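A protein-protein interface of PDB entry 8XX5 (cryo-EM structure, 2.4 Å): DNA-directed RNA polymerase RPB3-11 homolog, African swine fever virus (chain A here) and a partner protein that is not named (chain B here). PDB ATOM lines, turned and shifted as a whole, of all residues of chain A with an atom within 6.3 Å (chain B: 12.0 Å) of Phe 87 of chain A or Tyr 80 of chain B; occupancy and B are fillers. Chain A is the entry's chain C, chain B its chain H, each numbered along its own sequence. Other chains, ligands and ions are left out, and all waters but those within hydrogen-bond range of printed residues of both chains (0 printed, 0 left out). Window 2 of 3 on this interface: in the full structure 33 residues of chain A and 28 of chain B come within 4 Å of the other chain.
CE of Met 1 of chain B touches O of Phe 87 of chain A, at 3.7 Å. Tyr 76 of chain B touches Phe 87 of chain A. Phe 87 of chain A touches Tyr 80 of chain B. CG of Phe 92 of chain A touches CE of Met 1 of chain B, 3.6 Å away. CD1 of Leu 2 of chain B touches CE2 of Phe 92 of chain A (3.96 Å). Met 1 of chain B touches Phe 151 of chain A. Phe 151 of chain A touches Leu 2 of chain B (CD1 to CD2, 3.7 Å). CZ of Phe 151 of chain A touches CB of Tyr 76 of chain B, 3.5 Å away. Phe 151 of chain A touches Arg 77 of chain B (CG to CD, 3.7 Å). Tyr 80 of chain B touches Gln 153 of chain A (CE2 to OE1, 3.7 Å).
N of Phe 87 of chain A is in hydrogen-bond range of OD2 of Asp 85 of chain A, at 3.0 Å. The side-chain carboxylate of Asp 85 of chain A is in hydrogen-bond range of the backbone NH of Gln 153 of chain A (3.0 Å). The side-chain sulfur (SD) of Met 88 of chain A lies within hydrogen-bond range of the backbone NH (N) of Phe 151 of chain A (3.6 Å). OG1 of Thr 89 of chain A sits at hydrogen-bond distance from N of Phe 92 of chain A. The backbone NH (N) of Tyr 76 of chain B lies within hydrogen-bond range of the backbone carbonyl oxygen (O) of Met 1 of chain B, 2.7 Å away. The guanidinium group (NH1) of Arg 77 of chain B lies within salt-bridge range of the side-chain carboxylate (OD2) of Asp 75 of chain B (3.3 Å).
Hydrophobic or aromatic side chains of chain A within 4 Å of the printed part of chain B: Phe 87, Phe 92 and Phe 151. Of the 9 printed residues of chain B, 5 touch a printed residue of chain A. Printed residues of chain B that touch a printed residue of chain A: Met 1, Leu 2, Tyr 76, Arg 77 and Tyr 80. Hydrophobic or aromatic side chains of chain B within 4 Å of the printed part of chain A: Met 1, Leu 2, Tyr 76 and Tyr 80.
Of chain B, only Met 1, Tyr 76 and Tyr 80 come within 4 Å of Phe 87 of chain A. Tyr 80 of chain B touches just these residues of chain A: Phe 87 and Gln 153. Leu 86 of chain A touches none of the printed residues of chain B. Thr 89 of chain A touches none of the printed residues of chain B. Of the printed residues of chain A, Arg 77 of chain B touches Phe 151. Of the printed residues of chain B, Phe 92 of chain A touches Met 1 (3.6 Å) and Leu 2 (3.96 Å). Of the printed residues of chain A, Leu 2 of chain B touches Phe 92 (3.96 Å) and Phe 151 (3.7 Å). Of the printed residues of chain B, Gln 153 of chain A touches Tyr 80. Printed residues of chain A within 4 Å of Tyr 76 of chain B: Phe 87 and Phe 151. Thr 84 of chain A touches none of the printed residues of chain B. Asp 75 of chain B touches none of the printed residues of chain A. The nearest residue of chain A that does not touch Tyr 80 of chain B is Val 122 of chain A (5.2 Å). The nearest printed residue of chain A that does not touch Met 1 of chain B is Met 88 of chain A (4.4 Å).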
ATOM      1  N   THR A  84     -16.961  21.162 -33.863  1.00  0.00           N
ATOM      2  CA  THR A  84     -16.873  19.795 -33.371  1.00  0.00           C
ATOM      3  C   THR A  84     -17.863  19.506 -32.252  1.00  0.00           C
ATOM      4  O   THR A  84     -18.117  18.332 -31.961  1.00  0.00           O
ATOM      5  CB  THR A  84     -15.455  19.495 -32.882  1.00  0.00           C
ATOM      6  OG1 THR A  84     -14.978  20.590 -32.093  1.00  0.00           O
ATOM      7  CG2 THR A  84     -14.522  19.292 -34.060  1.00  0.00           C
ATOM      8  N   ASP A  85     -18.428  20.535 -31.626  1.00  0.00           N
ATOM      9  CA  ASP A  85     -19.351  20.316 -30.522  1.00  0.00           C
ATOM     10  C   ASP A  85     -20.616  19.633 -31.019  1.00  0.00           C
ATOM     11  O   ASP A  85     -21.179  20.010 -32.050  1.00  0.00           O
ATOM     12  CB  ASP A  85     -19.700  21.636 -29.839  1.00  0.00           C
ATOM     13  CG  ASP A  85     -20.349  21.431 -28.483  1.00  0.00           C
ATOM     14  OD1 ASP A  85     -19.616  21.222 -27.496  1.00  0.00           O
ATOM     15  OD2 ASP A  85     -21.593  21.474 -28.404  1.00  0.00           O
ATOM     16  N   LEU A  86     -21.062  18.626 -30.277  1.00  0.00           N
ATOM     17  CA  LEU A  86     -22.209  17.826 -30.669  1.00  0.00           C
ATOM     18  C   LEU A  86     -23.514  18.302 -30.048  1.00  0.00           C
ATOM     19  O   LEU A  86     -24.583  17.866 -30.487  1.00  0.00           O
ATOM     20  CB  LEU A  86     -21.966  16.361 -30.297  1.00  0.00           C
ATOM     21  CG  LEU A  86     -20.625  15.759 -30.718  1.00  0.00           C
ATOM     22  CD1 LEU A  86     -20.340  14.498 -29.925  1.00  0.00           C
ATOM     23  CD2 LEU A  86     -20.617  15.471 -32.208  1.00  0.00           C
ATOM     24  N   PHE A  87     -23.456  19.184 -29.053  1.00  0.00           N
ATOM     25  CA  PHE A  87     -24.654  19.670 -28.383  1.00  0.00           C
ATOM     26  C   PHE A  87     -25.070  21.062 -28.829  1.00  0.00           C
ATOM     27  O   PHE A  87     -26.262  21.380 -28.795  1.00  0.00           O
ATOM     28  CB  PHE A  87     -24.448  19.675 -26.866  1.00  0.00           C
ATOM     29  CG  PHE A  87     -24.310  18.307 -26.272  1.00  0.00           C
ATOM     30  CD1 PHE A  87     -23.077  17.681 -26.222  1.00  0.00           C
ATOM     31  CD2 PHE A  87     -25.414  17.644 -25.767  1.00  0.00           C
ATOM     32  CE1 PHE A  87     -22.948  16.421 -25.678  1.00  0.00           C
ATOM     33  CE2 PHE A  87     -25.290  16.384 -25.222  1.00  0.00           C
ATOM     34  CZ  PHE A  87     -24.057  15.772 -25.178  1.00  0.00           C
ATOM     35  N   MET A  88     -24.120  21.899 -29.246  1.00  0.00           N
ATOM     36  CA  MET A  88     -24.433  23.252 -29.702  1.00  0.00           C
ATOM     37  C   MET A  88     -24.818  23.186 -31.174  1.00  0.00           C
ATOM     38  O   MET A  88     -24.047  23.517 -32.077  1.00  0.00           O
ATOM     39  CB  MET A  88     -23.255  24.187 -29.464  1.00  0.00           C
ATOM     40  CG  MET A  88     -23.032  24.539 -28.006  1.00  0.00           C
ATOM     41  SD  MET A  88     -24.498  25.171 -27.170  1.00  0.00           S
ATOM     42  CE  MET A  88     -25.006  23.748 -26.211  1.00  0.00           C
ATOM     43  N   THR A  89     -26.049  22.741 -31.413  1.00  0.00           N
ATOM     44  CA  THR A  89     -26.550  22.614 -32.770  1.00  0.00           C
ATOM     45  C   THR A  89     -26.817  23.988 -33.374  1.00  0.00           C
ATOM     46  O   THR A  89     -26.944  24.994 -32.672  1.00  0.00           O
ATOM     47  CB  THR A  89     -27.825  21.771 -32.797  1.00  0.00           C
ATOM     48  OG1 THR A  89     -28.852  22.429 -32.047  1.00  0.00           O
ATOM     49  CG2 THR A  89     -27.566  20.404 -32.195  1.00  0.00           C
ATOM     50  N   PHE A  92     -30.095  25.632 -32.149  1.00  0.00           N
ATOM     51  CA  PHE A  92     -30.043  26.187 -30.801  1.00  0.00           C
ATOM     52  C   PHE A  92     -29.279  27.506 -30.774  1.00  0.00           C
ATOM     53  O   PHE A  92     -29.767  28.509 -30.240  1.00  0.00           O
ATOM     54  CB  PHE A  92     -29.409  25.173 -29.849  1.00  0.00           C
ATOM     55  CG  PHE A  92     -29.374  25.620 -28.418  1.00  0.00           C
ATOM     56  CD1 PHE A  92     -30.534  25.666 -27.665  1.00  0.00           C
ATOM     57  CD2 PHE A  92     -28.181  25.995 -27.825  1.00  0.00           C
ATOM     58  CE1 PHE A  92     -30.505  26.077 -26.349  1.00  0.00           C
ATOM     59  CE2 PHE A  92     -28.147  26.407 -26.509  1.00  0.00           C
ATOM     60  CZ  PHE A  92     -29.310  26.447 -25.770  1.00  0.00           C
ATOM     61  N   VAL A 122     -15.971  22.257 -19.138  1.00  0.00           N
ATOM     62  CA  VAL A 122     -17.001  22.759 -20.039  1.00  0.00           C
ATOM     63  C   VAL A 122     -16.907  24.278 -20.061  1.00  0.00           C
ATOM     64  O   VAL A 122     -17.002  24.932 -19.018  1.00  0.00           O
ATOM     65  CB  VAL A 122     -18.397  22.294 -19.603  1.00  0.00           C
ATOM     66  CG1 VAL A 122     -19.470  23.036 -20.381  1.00  0.00           C
ATOM     67  CG2 VAL A 122     -18.536  20.797 -19.796  1.00  0.00           C
ATOM     68  N   PHE A 151     -22.401  26.431 -24.549  1.00  0.00           N
ATOM     69  CA  PHE A 151     -21.310  25.823 -23.803  1.00  0.00           C
ATOM     70  C   PHE A 151     -20.648  24.749 -24.653  1.00  0.00           C
ATOM     71  O   PHE A 151     -21.300  24.079 -25.455  1.00  0.00           O
ATOM     72  CB  PHE A 151     -21.794  25.221 -22.475  1.00  0.00           C
ATOM     73  CG  PHE A 151     -23.025  24.372 -22.603  1.00  0.00           C
ATOM     74  CD1 PHE A 151     -24.286  24.937 -22.516  1.00  0.00           C
ATOM     75  CD2 PHE A 151     -22.923  23.007 -22.797  1.00  0.00           C
ATOM     76  CE1 PHE A 151     -25.418  24.158 -22.628  1.00  0.00           C
ATOM     77  CE2 PHE A 151     -24.052  22.224 -22.910  1.00  0.00           C
ATOM     78  CZ  PHE A 151     -25.301  22.800 -22.825  1.00  0.00           C
ATOM     79  N   GLN A 153     -18.258  21.292 -24.791  1.00  0.00           N
ATOM     80  CA  GLN A 153     -17.669  20.150 -24.124  1.00  0.00           C
ATOM     81  C   GLN A 153     -16.149  20.207 -24.264  1.00  0.00           C
ATOM     82  O   GLN A 153     -15.628  20.854 -25.175  1.00  0.00           O
ATOM     83  CB  GLN A 153     -18.207  18.850 -24.717  1.00  0.00           C
ATOM     84  CG  GLN A 153     -19.687  18.609 -24.480  1.00  0.00           C
ATOM     85  CD  GLN A 153     -20.094  18.817 -23.038  1.00  0.00           C
ATOM     86  OE1 GLN A 153     -19.507  18.239 -22.124  1.00  0.00           O
ATOM     87  NE2 GLN A 153     -21.111  19.643 -22.825  1.00  0.00           N
ATOM     88  N   MET B   1     -31.550  24.330 -22.926  1.00  0.00           N
ATOM     89  CA  MET B   1     -30.338  23.852 -22.274  1.00  0.00           C
ATOM     90  C   MET B   1     -29.692  24.946 -21.435  1.00  0.00           C
ATOM     91  O   MET B   1     -28.782  24.688 -20.649  1.00  0.00           O
ATOM     92  CB  MET B   1     -29.347  23.323 -23.310  1.00  0.00           C
ATOM     93  CG  MET B   1     -29.868  22.147 -24.117  1.00  0.00           C
ATOM     94  SD  MET B   1     -28.669  21.535 -25.311  1.00  0.00           S
ATOM     95  CE  MET B   1     -29.148  22.451 -26.769  1.00  0.00           C
ATOM     96  N   LEU B   2     -30.170  26.174 -21.614  1.00  0.00           N
ATOM     97  CA  LEU B   2     -29.700  27.323 -20.859  1.00  0.00           C
ATOM     98  C   LEU B   2     -30.900  28.181 -20.499  1.00  0.00           C
ATOM     99  O   LEU B   2     -31.999  27.998 -21.029  1.00  0.00           O
ATOM    100  CB  LEU B   2     -28.680  28.150 -21.654  1.00  0.00           C
ATOM    101  CG  LEU B   2     -27.359  27.492 -22.047  1.00  0.00           C
ATOM    102  CD1 LEU B   2     -26.755  28.187 -23.252  1.00  0.00           C
ATOM    103  CD2 LEU B   2     -26.391  27.516 -20.883  1.00  0.00           C
ATOM    104  N   LEU B  74     -33.873  24.976 -16.599  1.00  0.00           N
ATOM    105  CA  LEU B  74     -32.825  24.020 -16.284  1.00  0.00           C
ATOM    106  C   LEU B  74     -31.586  24.278 -17.130  1.00  0.00           C
ATOM    107  O   LEU B  74     -31.680  24.562 -18.327  1.00  0.00           O
ATOM    108  CB  LEU B  74     -33.319  22.593 -16.512  1.00  0.00           C
ATOM    109  CG  LEU B  74     -34.601  22.195 -15.790  1.00  0.00           C
ATOM    110  CD1 LEU B  74     -35.012  20.796 -16.199  1.00  0.00           C
ATOM    111  CD2 LEU B  74     -34.419  22.288 -14.288  1.00  0.00           C
ATOM    112  N   ASP B  75     -30.423  24.175 -16.499  1.00  0.00           N
ATOM    113  CA  ASP B  75     -29.145  24.306 -17.181  1.00  0.00           C
ATOM    114  C   ASP B  75     -28.630  22.920 -17.538  1.00  0.00           C
ATOM    115  O   ASP B  75     -28.511  22.054 -16.665  1.00  0.00           O
ATOM    116  CB  ASP B  75     -28.131  25.042 -16.306  1.00  0.00           C
ATOM    117  CG  ASP B  75     -26.991  25.631 -17.107  1.00  0.00           C
ATOM    118  OD1 ASP B  75     -26.927  25.382 -18.328  1.00  0.00           O
ATOM    119  OD2 ASP B  75     -26.155  26.344 -16.514  1.00  0.00           O
ATOM    120  N   TYR B  76     -28.327  22.715 -18.820  1.00  0.00           N
ATOM    121  CA  TYR B  76     -27.908  21.397 -19.285  1.00  0.00           C
ATOM    122  C   TYR B  76     -26.575  20.982 -18.678  1.00  0.00           C
ATOM    123  O   TYR B  76     -26.384  19.810 -18.335  1.00  0.00           O
ATOM    124  CB  TYR B  76     -27.827  21.384 -20.809  1.00  0.00           C
ATOM    125  CG  TYR B  76     -27.929  20.011 -21.429  1.00  0.00           C
ATOM    126  CD1 TYR B  76     -29.159  19.394 -21.596  1.00  0.00           C
ATOM    127  CD2 TYR B  76     -26.794  19.337 -21.858  1.00  0.00           C
ATOM    128  CE1 TYR B  76     -29.257  18.144 -22.166  1.00  0.00           C
ATOM    129  CE2 TYR B  76     -26.882  18.086 -22.429  1.00  0.00           C
ATOM    130  CZ  TYR B  76     -28.116  17.494 -22.581  1.00  0.00           C
ATOM    131  OH  TYR B  76     -28.208  16.248 -23.150  1.00  0.00           O
ATOM    132  N   ARG B  77     -25.636  21.921 -18.538  1.00  0.00           N
ATOM    133  CA  ARG B  77     -24.317  21.557 -18.037  1.00  0.00           C
ATOM    134  C   ARG B  77     -24.345  21.128 -16.577  1.00  0.00           C
ATOM    135  O   ARG B  77     -23.397  20.486 -16.117  1.00  0.00           O
ATOM    136  CB  ARG B  77     -23.328  22.711 -18.211  1.00  0.00           C
ATOM    137  CG  ARG B  77     -23.932  24.094 -18.175  1.00  0.00           C
ATOM    138  CD  ARG B  77     -23.110  25.055 -19.013  1.00  0.00           C
ATOM    139  NE  ARG B  77     -23.750  26.358 -19.141  1.00  0.00           N
ATOM    140  CZ  ARG B  77     -23.702  27.305 -18.216  1.00  0.00           C
ATOM    141  NH1 ARG B  77     -23.041  27.133 -17.084  1.00  0.00           N
ATOM    142  NH2 ARG B  77     -24.330  28.456 -18.432  1.00  0.00           N
ATOM    143  N   LYS B  78     -25.400  21.465 -15.840  1.00  0.00           N
ATOM    144  CA  LYS B  78     -25.536  21.025 -14.461  1.00  0.00           C
ATOM    145  C   LYS B  78     -26.091  19.613 -14.341  1.00  0.00           C
ATOM    146  O   LYS B  78     -26.007  19.021 -13.260  1.00  0.00           O
ATOM    147  CB  LYS B  78     -26.430  21.996 -13.687  1.00  0.00           C
ATOM    148  CG  LYS B  78     -25.850  23.387 -13.585  1.00  0.00           C
ATOM    149  CD  LYS B  78     -26.859  24.367 -13.035  1.00  0.00           C
ATOM    150  CE  LYS B  78     -26.223  25.726 -12.834  1.00  0.00           C
ATOM    151  NZ  LYS B  78     -25.017  25.899 -13.691  1.00  0.00           N
ATOM    152  N   TYR B  79     -26.651  19.063 -15.417  1.00  0.00           N
ATOM    153  CA  TYR B  79     -27.122  17.689 -15.438  1.00  0.00           C
ATOM    154  C   TYR B  79     -26.310  16.796 -16.362  1.00  0.00           C
ATOM    155  O   TYR B  79     -26.469  15.573 -16.310  1.00  0.00           O
ATOM    156  CB  TYR B  79     -28.598  17.637 -15.855  1.00  0.00           C
ATOM    157  CG  TYR B  79     -29.509  18.438 -14.958  1.00  0.00           C
ATOM    158  CD1 TYR B  79     -29.940  17.929 -13.742  1.00  0.00           C
ATOM    159  CD2 TYR B  79     -29.931  19.707 -15.322  1.00  0.00           C
ATOM    160  CE1 TYR B  79     -30.770  18.659 -12.918  1.00  0.00           C
ATOM    161  CE2 TYR B  79     -30.760  20.444 -14.504  1.00  0.00           C
ATOM    162  CZ  TYR B  79     -31.178  19.916 -13.303  1.00  0.00           C
ATOM    163  OH  TYR B  79     -32.004  20.649 -12.484  1.00  0.00           O
ATOM    164  N   TYR B  80     -25.452  17.366 -17.198  1.00  0.00           N
ATOM    165  CA  TYR B  80     -24.605  16.584 -18.084  1.00  0.00           C
ATOM    166  C   TYR B  80     -23.139  16.910 -17.835  1.00  0.00           C
ATOM    167  O   TYR B  80     -22.619  17.909 -18.329  1.00  0.00           O
ATOM    168  CB  TYR B  80     -24.970  16.847 -19.544  1.00  0.00           C
ATOM    169  CG  TYR B  80     -24.183  16.023 -20.535  1.00  0.00           C
ATOM    170  CD1 TYR B  80     -24.544  14.715 -20.820  1.00  0.00           C
ATOM    171  CD2 TYR B  80     -23.083  16.558 -21.191  1.00  0.00           C
ATOM    172  CE1 TYR B  80     -23.829  13.962 -21.726  1.00  0.00           C
ATOM    173  CE2 TYR B  80     -22.362  15.812 -22.096  1.00  0.00           C
ATOM    174  CZ  TYR B  80     -22.740  14.517 -22.363  1.00  0.00           C
ATOM    175  OH  TYR B  80     -22.023  13.771 -23.266  1.00  0.00           O
ATOM    176  OXT TYR B  80     -22.439  16.181 -17.133  1.00  0.00           O
